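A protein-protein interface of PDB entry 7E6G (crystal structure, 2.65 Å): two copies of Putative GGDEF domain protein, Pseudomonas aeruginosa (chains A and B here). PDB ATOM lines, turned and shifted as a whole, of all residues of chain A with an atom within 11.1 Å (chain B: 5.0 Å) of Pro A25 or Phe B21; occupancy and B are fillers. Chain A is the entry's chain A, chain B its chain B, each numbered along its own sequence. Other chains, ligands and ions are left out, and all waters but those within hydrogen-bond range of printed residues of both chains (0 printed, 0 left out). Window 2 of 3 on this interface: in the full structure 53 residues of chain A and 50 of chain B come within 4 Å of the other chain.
Hydrophobic or aromatic side chains of chain B that line the printed part of chain A: Leu B15, Phe B21 and His B24.
Of the 17 printed residues of chain A, 4 touch a printed residue of chain B.
Printed residues of chain A that touch a printed residue of chain B: Phe A21, His A24, Pro A25 and Leu A26.
Among the printed residues, no Asp or Glu carboxylate lies within 4 Å of a Lys or Arg side-chain nitrogen of the other chain.
The backbone NH of Leu A26 is in hydrogen-bond range of a ring nitrogen (ND1) of His A24, at 3.0 Å.
Phe A21 touches His B24, and with the chains exchanged His A24 touches Phe B21.
His B24 touches its own counterpart, His A24.
NE2 of His A24 is in hydrogen-bond range of NE2 of His B24, 2.8 Å away.
Pro A25 touches just one residue of chain B: Phe B21 (3.8 Å).
Of the printed residues of chain A, Phe B21 touches His A24 (3.6 Å), Pro A25 (3.8 Å) and Leu A26 (3.8 Å).
No residue of chain A comes within 4 Å of Asp B18.
No residue of chain A comes within 4 Å of Pro B19.
No residue of chain A comes within 4 Å of Gln B20.
No residue of chain A comes within 4 Å of His B22.
Gly B23 touches none of the printed residues of chain A.
His B24 touches two residues of chain A.
Printed residues of chain B within 4 Å of Leu A26: Leu B15, Phe B21 and His B27.
Printed residues of chain B within 4 Å of His A24: Phe B21 and His B24.
Of the printed residues of chain B, Phe A21 touches His B24.
Ala A29 touches none of the printed residues of chain B.
Leu A30 touches none of the printed residues of chain B.
The nearest residue of chain B that does not touch Pro A25 is Leu B15 (4.8 Å).
The nearest residue of chain A that does not touch Phe B21 is His A27 (8.0 Å).
Among the printed residues, pairs that only touch across the chains: Phe A21 with His B24 (3.5 Å), His A24 with Phe B21 (3.6 Å), Pro A25 with Phe B21 (3.8 Å), Leu A26 with Leu B15 (3.6 Å), Leu A26 with Phe B21 (3.8 Å) and Leu A26 with His B27 (3.6 Å).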
ATOM      1  N   TRP A  11     -18.397  21.976 -30.731  1.00  0.00           N
ATOM      2  CA  TRP A  11     -19.722  21.590 -30.244  1.00  0.00           C
ATOM      3  C   TRP A  11     -19.621  20.517 -29.163  1.00  0.00           C
ATOM      4  O   TRP A  11     -20.287  20.595 -28.123  1.00  0.00           O
ATOM      5  CB  TRP A  11     -20.580  21.106 -31.410  1.00  0.00           C
ATOM      6  CG  TRP A  11     -21.959  20.697 -30.980  1.00  0.00           C
ATOM      7  CD1 TRP A  11     -22.830  21.427 -30.224  1.00  0.00           C
ATOM      8  CD2 TRP A  11     -22.619  19.447 -31.254  1.00  0.00           C
ATOM      9  NE1 TRP A  11     -23.992  20.721 -30.023  1.00  0.00           N
ATOM     10  CE2 TRP A  11     -23.886  19.501 -30.638  1.00  0.00           C
ATOM     11  CE3 TRP A  11     -22.260  18.292 -31.960  1.00  0.00           C
ATOM     12  CZ2 TRP A  11     -24.800  18.446 -30.709  1.00  0.00           C
ATOM     13  CZ3 TRP A  11     -23.173  17.241 -32.035  1.00  0.00           C
ATOM     14  CH2 TRP A  11     -24.424  17.325 -31.412  1.00  0.00           C
ATOM     15  N   LEU A  16     -19.611  18.569 -23.493  1.00  0.00           N
ATOM     16  CA  LEU A  16     -18.919  17.890 -22.404  1.00  0.00           C
ATOM     17  C   LEU A  16     -18.756  18.791 -21.197  1.00  0.00           C
ATOM     18  O   LEU A  16     -18.677  18.291 -20.068  1.00  0.00           O
ATOM     19  CB  LEU A  16     -17.554  17.400 -22.873  1.00  0.00           C
ATOM     20  CG  LEU A  16     -17.607  16.195 -23.802  1.00  0.00           C
ATOM     21  CD1 LEU A  16     -16.240  15.941 -24.431  1.00  0.00           C
ATOM     22  CD2 LEU A  16     -18.131  14.969 -23.048  1.00  0.00           C
ATOM     23  N   PRO A  19     -22.967  21.414 -17.440  1.00  0.00           N
ATOM     24  CA  PRO A  19     -23.216  20.623 -16.217  1.00  0.00           C
ATOM     25  C   PRO A  19     -24.462  19.759 -16.274  1.00  0.00           C
ATOM     26  O   PRO A  19     -24.564  18.793 -15.499  1.00  0.00           O
ATOM     27  CB  PRO A  19     -23.329  21.695 -15.122  1.00  0.00           C
ATOM     28  CG  PRO A  19     -22.576  22.852 -15.657  1.00  0.00           C
ATOM     29  CD  PRO A  19     -22.822  22.850 -17.142  1.00  0.00           C
ATOM     30  N   GLN A  20     -25.408  20.050 -17.170  1.00  0.00           N
ATOM     31  CA  GLN A  20     -26.626  19.248 -17.206  1.00  0.00           C
ATOM     32  C   GLN A  20     -26.379  17.824 -17.696  1.00  0.00           C
ATOM     33  O   GLN A  20     -27.203  16.943 -17.423  1.00  0.00           O
ATOM     34  CB  GLN A  20     -27.673  19.930 -18.075  1.00  0.00           C
ATOM     35  CG  GLN A  20     -27.621  19.536 -19.523  1.00  0.00           C
ATOM     36  CD  GLN A  20     -28.510  20.403 -20.378  1.00  0.00           C
ATOM     37  OE1 GLN A  20     -28.036  21.338 -21.031  1.00  0.00           O
ATOM     38  NE2 GLN A  20     -29.812  20.100 -20.380  1.00  0.00           N
ATOM     39  N   PHE A  21     -25.265  17.601 -18.417  1.00  0.00           N
ATOM     40  CA  PHE A  21     -24.899  16.315 -18.938  1.00  0.00           C
ATOM     41  C   PHE A  21     -24.008  15.479 -18.145  1.00  0.00           C
ATOM     42  O   PHE A  21     -23.956  14.355 -18.352  1.00  0.00           O
ATOM     43  CB  PHE A  21     -24.356  16.411 -20.305  1.00  0.00           C
ATOM     44  CG  PHE A  21     -25.238  17.062 -21.241  1.00  0.00           C
ATOM     45  CD1 PHE A  21     -26.494  16.636 -21.429  1.00  0.00           C
ATOM     46  CD2 PHE A  21     -24.796  18.091 -21.955  1.00  0.00           C
ATOM     47  CE1 PHE A  21     -27.305  17.258 -22.279  1.00  0.00           C
ATOM     48  CE2 PHE A  21     -25.608  18.726 -22.830  1.00  0.00           C
ATOM     49  CZ  PHE A  21     -26.844  18.280 -23.001  1.00  0.00           C
ATOM     50  N   HIS A  22     -23.389  16.043 -17.178  1.00  0.00           N
ATOM     51  CA  HIS A  22     -22.487  15.355 -16.349  1.00  0.00           C
ATOM     52  C   HIS A  22     -23.269  14.345 -15.624  1.00  0.00           C
ATOM     53  O   HIS A  22     -24.200  14.640 -15.056  1.00  0.00           O
ATOM     54  CB  HIS A  22     -21.822  16.391 -15.489  1.00  0.00           C
ATOM     55  CG  HIS A  22     -21.009  17.415 -16.254  1.00  0.00           C
ATOM     56  ND1 HIS A  22     -20.246  18.388 -15.661  1.00  0.00           N
ATOM     57  CD2 HIS A  22     -20.849  17.616 -17.564  1.00  0.00           C
ATOM     58  CE1 HIS A  22     -19.676  19.139 -16.559  1.00  0.00           C
ATOM     59  NE2 HIS A  22     -20.000  18.664 -17.722  1.00  0.00           N
ATOM     60  N   GLY A  23     -22.869  13.120 -15.641  1.00  0.00           N
ATOM     61  CA  GLY A  23     -23.617  12.032 -15.066  1.00  0.00           C
ATOM     62  C   GLY A  23     -24.458  11.177 -15.974  1.00  0.00           C
ATOM     63  O   GLY A  23     -24.721  10.095 -15.673  1.00  0.00           O
ATOM     64  N   HIS A  24     -24.747  11.618 -17.168  1.00  0.00           N
ATOM     65  CA  HIS A  24     -25.513  10.904 -18.137  1.00  0.00           C
ATOM     66  C   HIS A  24     -24.806   9.741 -18.616  1.00  0.00           C
ATOM     67  O   HIS A  24     -23.678   9.702 -18.695  1.00  0.00           O
ATOM     68  CB  HIS A  24     -25.714  11.820 -19.242  1.00  0.00           C
ATOM     69  CG  HIS A  24     -26.736  11.412 -20.221  1.00  0.00           C
ATOM     70  ND1 HIS A  24     -26.634  10.328 -21.008  1.00  0.00           N
ATOM     71  CD2 HIS A  24     -27.836  12.028 -20.618  1.00  0.00           C
ATOM     72  CE1 HIS A  24     -27.670  10.234 -21.771  1.00  0.00           C
ATOM     73  NE2 HIS A  24     -28.417  11.258 -21.551  1.00  0.00           N
ATOM     74  N   PRO A  25     -25.480   8.747 -18.993  1.00  0.00           N
ATOM     75  CA  PRO A  25     -24.738   7.537 -19.400  1.00  0.00           C
ATOM     76  C   PRO A  25     -23.907   7.703 -20.664  1.00  0.00           C
ATOM     77  O   PRO A  25     -23.005   6.884 -20.893  1.00  0.00           O
ATOM     78  CB  PRO A  25     -25.849   6.497 -19.605  1.00  0.00           C
ATOM     79  CG  PRO A  25     -26.972   6.983 -18.776  1.00  0.00           C
ATOM     80  CD  PRO A  25     -26.915   8.478 -18.808  1.00  0.00           C
ATOM     81  N   LEU A  26     -24.102   8.744 -21.400  1.00  0.00           N
ATOM     82  CA  LEU A  26     -23.368   8.978 -22.572  1.00  0.00           C
ATOM     83  C   LEU A  26     -22.330   9.981 -22.536  1.00  0.00           C
ATOM     84  O   LEU A  26     -21.771  10.176 -23.470  1.00  0.00           O
ATOM     85  CB  LEU A  26     -24.286   9.302 -23.695  1.00  0.00           C
ATOM     86  CG  LEU A  26     -25.405   8.482 -24.205  1.00  0.00           C
ATOM     87  CD1 LEU A  26     -25.923   9.019 -25.440  1.00  0.00           C
ATOM     88  CD2 LEU A  26     -25.121   7.091 -24.329  1.00  0.00           C
ATOM     89  N   HIS A  27     -22.111  10.644 -21.452  1.00  0.00           N
ATOM     90  CA  HIS A  27     -21.106  11.628 -21.319  1.00  0.00           C
ATOM     91  C   HIS A  27     -19.701  11.194 -21.353  1.00  0.00           C
ATOM     92  O   HIS A  27     -18.966  11.562 -22.098  1.00  0.00           O
ATOM     93  CB  HIS A  27     -21.353  12.292 -20.040  1.00  0.00           C
ATOM     94  CG  HIS A  27     -20.487  13.453 -19.799  1.00  0.00           C
ATOM     95  ND1 HIS A  27     -19.387  13.388 -19.025  1.00  0.00           N
ATOM     96  CD2 HIS A  27     -20.540  14.698 -20.254  1.00  0.00           C
ATOM     97  CE1 HIS A  27     -18.766  14.520 -19.059  1.00  0.00           C
ATOM     98  NE2 HIS A  27     -19.462  15.344 -19.767  1.00  0.00           N
ATOM     99  N   GLN A  28     -19.438  10.223 -20.595  1.00  0.00           N
ATOM    100  CA  GLN A  28     -18.183   9.611 -20.444  1.00  0.00           C
ATOM    101  C   GLN A  28     -17.799   8.893 -21.694  1.00  0.00           C
ATOM    102  O   GLN A  28     -16.764   8.741 -21.922  1.00  0.00           O
ATOM    103  CB  GLN A  28     -18.178   8.810 -19.170  1.00  0.00           C
ATOM    104  CG  GLN A  28     -16.893   8.613 -18.446  1.00  0.00           C
ATOM    105  CD  GLN A  28     -16.512   7.140 -18.372  1.00  0.00           C
ATOM    106  OE1 GLN A  28     -15.774   6.728 -17.528  1.00  0.00           O
ATOM    107  NE2 GLN A  28     -17.070   6.349 -19.226  1.00  0.00           N
ATOM    108  N   ALA A  29     -18.705   8.333 -22.401  1.00  0.00           N
ATOM    109  CA  ALA A  29     -18.547   7.744 -23.654  1.00  0.00           C
ATOM    110  C   ALA A  29     -18.150   8.694 -24.699  1.00  0.00           C
ATOM    111  O   ALA A  29     -17.382   8.395 -25.409  1.00  0.00           O
ATOM    112  CB  ALA A  29     -19.823   7.125 -23.961  1.00  0.00           C
ATOM    113  N   LEU A  30     -18.726   9.839 -24.761  1.00  0.00           N
ATOM    114  CA  LEU A  30     -18.384  10.846 -25.664  1.00  0.00           C
ATOM    115  C   LEU A  30     -17.107  11.413 -25.404  1.00  0.00           C
ATOM    116  O   LEU A  30     -16.532  11.828 -26.259  1.00  0.00           O
ATOM    117  CB  LEU A  30     -19.426  11.879 -25.808  1.00  0.00           C
ATOM    118  CG  LEU A  30     -19.154  12.973 -26.764  1.00  0.00           C
ATOM    119  CD1 LEU A  30     -19.225  12.662 -28.176  1.00  0.00           C
ATOM    120  CD2 LEU A  30     -20.044  14.077 -26.596  1.00  0.00           C
ATOM    121  N   ALA A  31     -16.709  11.586 -24.192  1.00  0.00           N
ATOM    122  CA  ALA A  31     -15.354  12.051 -23.886  1.00  0.00           C
ATOM    123  C   ALA A  31     -14.312  11.058 -24.393  1.00  0.00           C
ATOM    124  O   ALA A  31     -13.314  11.440 -25.036  1.00  0.00           O
ATOM    125  CB  ALA A  31     -15.198  12.280 -22.377  1.00  0.00           C
ATOM    126  N   ARG A  32     -14.545   9.767 -24.127  1.00  0.00           N
ATOM    127  CA  ARG A  32     -13.609   8.742 -24.568  1.00  0.00           C
ATOM    128  C   ARG A  32     -13.516   8.707 -26.082  1.00  0.00           C
ATOM    129  O   ARG A  32     -12.420   8.614 -26.644  1.00  0.00           O
ATOM    130  CB  ARG A  32     -14.023   7.380 -24.019  1.00  0.00           C
ATOM    131  CG  ARG A  32     -13.810   7.284 -22.541  1.00  0.00           C
ATOM    132  CD  ARG A  32     -14.354   6.004 -21.979  1.00  0.00           C
ATOM    133  NE  ARG A  32     -13.647   4.854 -22.512  1.00  0.00           N
ATOM    134  CZ  ARG A  32     -13.733   3.638 -21.999  1.00  0.00           C
ATOM    135  NH1 ARG A  32     -14.503   3.421 -20.936  1.00  0.00           N
ATOM    136  NH2 ARG A  32     -13.055   2.644 -22.557  1.00  0.00           N
ATOM    137  N   LEU A  33     -14.646   8.838 -26.765  1.00  0.00           N
ATOM    138  CA  LEU A  33     -14.601   8.713 -28.212  1.00  0.00           C
ATOM    139  C   LEU A  33     -14.013   9.960 -28.864  1.00  0.00           C
ATOM    140  O   LEU A  33     -13.286   9.855 -29.859  1.00  0.00           O
ATOM    141  CB  LEU A  33     -15.980   8.380 -28.762  1.00  0.00           C
ATOM    142  CG  LEU A  33     -15.961   8.149 -30.267  1.00  0.00           C
ATOM    143  CD1 LEU A  33     -15.728   6.693 -30.583  1.00  0.00           C
ATOM    144  CD2 LEU A  33     -17.290   8.559 -30.761  1.00  0.00           C
ATOM    145  N   LEU B  15     -24.531   1.494 -27.299  1.00  0.00           N
ATOM    146  CA  LEU B  15     -25.205   2.651 -26.715  1.00  0.00           C
ATOM    147  C   LEU B  15     -26.115   3.328 -27.741  1.00  0.00           C
ATOM    148  O   LEU B  15     -27.281   3.622 -27.458  1.00  0.00           O
ATOM    149  CB  LEU B  15     -24.164   3.636 -26.170  1.00  0.00           C
ATOM    150  CG  LEU B  15     -23.837   3.706 -24.673  1.00  0.00           C
ATOM    151  CD1 LEU B  15     -24.436   2.547 -23.897  1.00  0.00           C
ATOM    152  CD2 LEU B  15     -22.341   3.741 -24.497  1.00  0.00           C
ATOM    153  N   ASP B  18     -29.574   2.082 -28.352  1.00  0.00           N
ATOM    154  CA  ASP B  18     -30.551   2.140 -27.269  1.00  0.00           C
ATOM    155  C   ASP B  18     -31.524   3.277 -27.560  1.00  0.00           C
ATOM    156  O   ASP B  18     -31.128   4.449 -27.526  1.00  0.00           O
ATOM    157  CB  ASP B  18     -29.864   2.336 -25.915  1.00  0.00           C
ATOM    158  CG  ASP B  18     -30.817   2.167 -24.738  1.00  0.00           C
ATOM    159  OD1 ASP B  18     -32.002   2.600 -24.827  1.00  0.00           O
ATOM    160  OD2 ASP B  18     -30.354   1.623 -23.704  1.00  0.00           O
ATOM    161  N   PRO B  19     -32.797   2.978 -27.839  1.00  0.00           N
ATOM    162  CA  PRO B  19     -33.724   4.041 -28.256  1.00  0.00           C
ATOM    163  C   PRO B  19     -33.970   5.083 -27.191  1.00  0.00           C
ATOM    164  O   PRO B  19     -34.520   6.147 -27.509  1.00  0.00           O
ATOM    165  CB  PRO B  19     -35.017   3.284 -28.585  1.00  0.00           C
ATOM    166  CG  PRO B  19     -34.643   1.878 -28.687  1.00  0.00           C
ATOM    167  CD  PRO B  19     -33.448   1.664 -27.809  1.00  0.00           C
ATOM    168  N   GLN B  20     -33.611   4.827 -25.932  1.00  0.00           N
ATOM    169  CA  GLN B  20     -33.912   5.835 -24.922  1.00  0.00           C
ATOM    170  C   GLN B  20     -33.054   7.073 -25.114  1.00  0.00           C
ATOM    171  O   GLN B  20     -33.461   8.167 -24.706  1.00  0.00           O
ATOM    172  CB  GLN B  20     -33.737   5.270 -23.516  1.00  0.00           C
ATOM    173  CG  GLN B  20     -32.315   5.259 -23.032  1.00  0.00           C
ATOM    174  CD  GLN B  20     -32.180   4.607 -21.678  1.00  0.00           C
ATOM    175  OE1 GLN B  20     -31.470   3.606 -21.531  1.00  0.00           O
ATOM    176  NE2 GLN B  20     -32.875   5.164 -20.675  1.00  0.00           N
ATOM    177  N   PHE B  21     -31.889   6.928 -25.760  1.00  0.00           N
ATOM    178  CA  PHE B  21     -31.002   8.051 -26.022  1.00  0.00           C
ATOM    179  C   PHE B  21     -31.236   8.695 -27.377  1.00  0.00           C
ATOM    180  O   PHE B  21     -30.648   9.748 -27.650  1.00  0.00           O
ATOM    181  CB  PHE B  21     -29.543   7.607 -25.915  1.00  0.00           C
ATOM    182  CG  PHE B  21     -29.211   6.957 -24.596  1.00  0.00           C
ATOM    183  CD1 PHE B  21     -29.498   7.607 -23.392  1.00  0.00           C
ATOM    184  CD2 PHE B  21     -28.633   5.687 -24.550  1.00  0.00           C
ATOM    185  CE1 PHE B  21     -29.199   7.004 -22.163  1.00  0.00           C
ATOM    186  CE2 PHE B  21     -28.334   5.078 -23.323  1.00  0.00           C
ATOM    187  CZ  PHE B  21     -28.618   5.738 -22.131  1.00  0.00           C
ATOM    188  N   HIS B  22     -32.025   8.171 -28.224  1.00  0.00           N
ATOM    189  CA  HIS B  22     -32.231   8.756 -29.459  1.00  0.00           C
ATOM    190  C   HIS B  22     -32.668  10.158 -29.330  1.00  0.00           C
ATOM    191  O   HIS B  22     -33.426  10.453 -28.559  1.00  0.00           O
ATOM    192  CB  HIS B  22     -33.281   7.957 -30.074  1.00  0.00           C
ATOM    193  CG  HIS B  22     -32.829   6.725 -30.741  1.00  0.00           C
ATOM    194  ND1 HIS B  22     -33.648   6.001 -31.550  1.00  0.00           N
ATOM    195  CD2 HIS B  22     -31.675   6.081 -30.741  1.00  0.00           C
ATOM    196  CE1 HIS B  22     -33.027   4.955 -32.003  1.00  0.00           C
ATOM    197  NE2 HIS B  22     -31.820   4.982 -31.537  1.00  0.00           N
ATOM    198  N   GLY B  23     -32.168  11.032 -30.137  1.00  0.00           N
ATOM    199  CA  GLY B  23     -32.480  12.446 -30.098  1.00  0.00           C
ATOM    200  C   GLY B  23     -31.661  13.246 -29.108  1.00  0.00           C
ATOM    201  O   GLY B  23     -31.464  14.455 -29.306  1.00  0.00           O
ATOM    202  N   HIS B  24     -31.181  12.599 -28.045  1.00  0.00           N
ATOM    203  CA  HIS B  24     -30.333  13.271 -27.069  1.00  0.00           C
ATOM    204  C   HIS B  24     -29.125  13.896 -27.766  1.00  0.00           C
ATOM    205  O   HIS B  24     -28.591  13.323 -28.727  1.00  0.00           O
ATOM    206  CB  HIS B  24     -29.873  12.279 -26.001  1.00  0.00           C
ATOM    207  CG  HIS B  24     -29.361  12.924 -24.753  1.00  0.00           C
ATOM    208  ND1 HIS B  24     -28.098  13.472 -24.661  1.00  0.00           N
ATOM    209  CD2 HIS B  24     -29.940  13.101 -23.542  1.00  0.00           C
ATOM    210  CE1 HIS B  24     -27.925  13.964 -23.448  1.00  0.00           C
ATOM    211  NE2 HIS B  24     -29.027  13.754 -22.750  1.00  0.00           N
ATOM    212  N   HIS B  27     -26.100  11.626 -27.891  1.00  0.00           N
ATOM    213  CA  HIS B  27     -26.311  10.617 -28.926  1.00  0.00           C
ATOM    214  C   HIS B  27     -25.969  11.161 -30.308  1.00  0.00           C
ATOM    215  O   HIS B  27     -25.283  10.498 -31.098  1.00  0.00           O
ATOM    216  CB  HIS B  27     -27.762  10.146 -28.884  1.00  0.00           C
ATOM    217  CG  HIS B  27     -28.086   9.082 -29.884  1.00  0.00           C
ATOM    218  ND1 HIS B  27     -28.333   9.358 -31.213  1.00  0.00           N
ATOM    219  CD2 HIS B  27     -28.213   7.740 -29.747  1.00  0.00           C
ATOM    220  CE1 HIS B  27     -28.597   8.231 -31.849  1.00  0.00           C
ATOM    221  NE2 HIS B  27     -28.536   7.236 -30.982  1.00  0.00           N
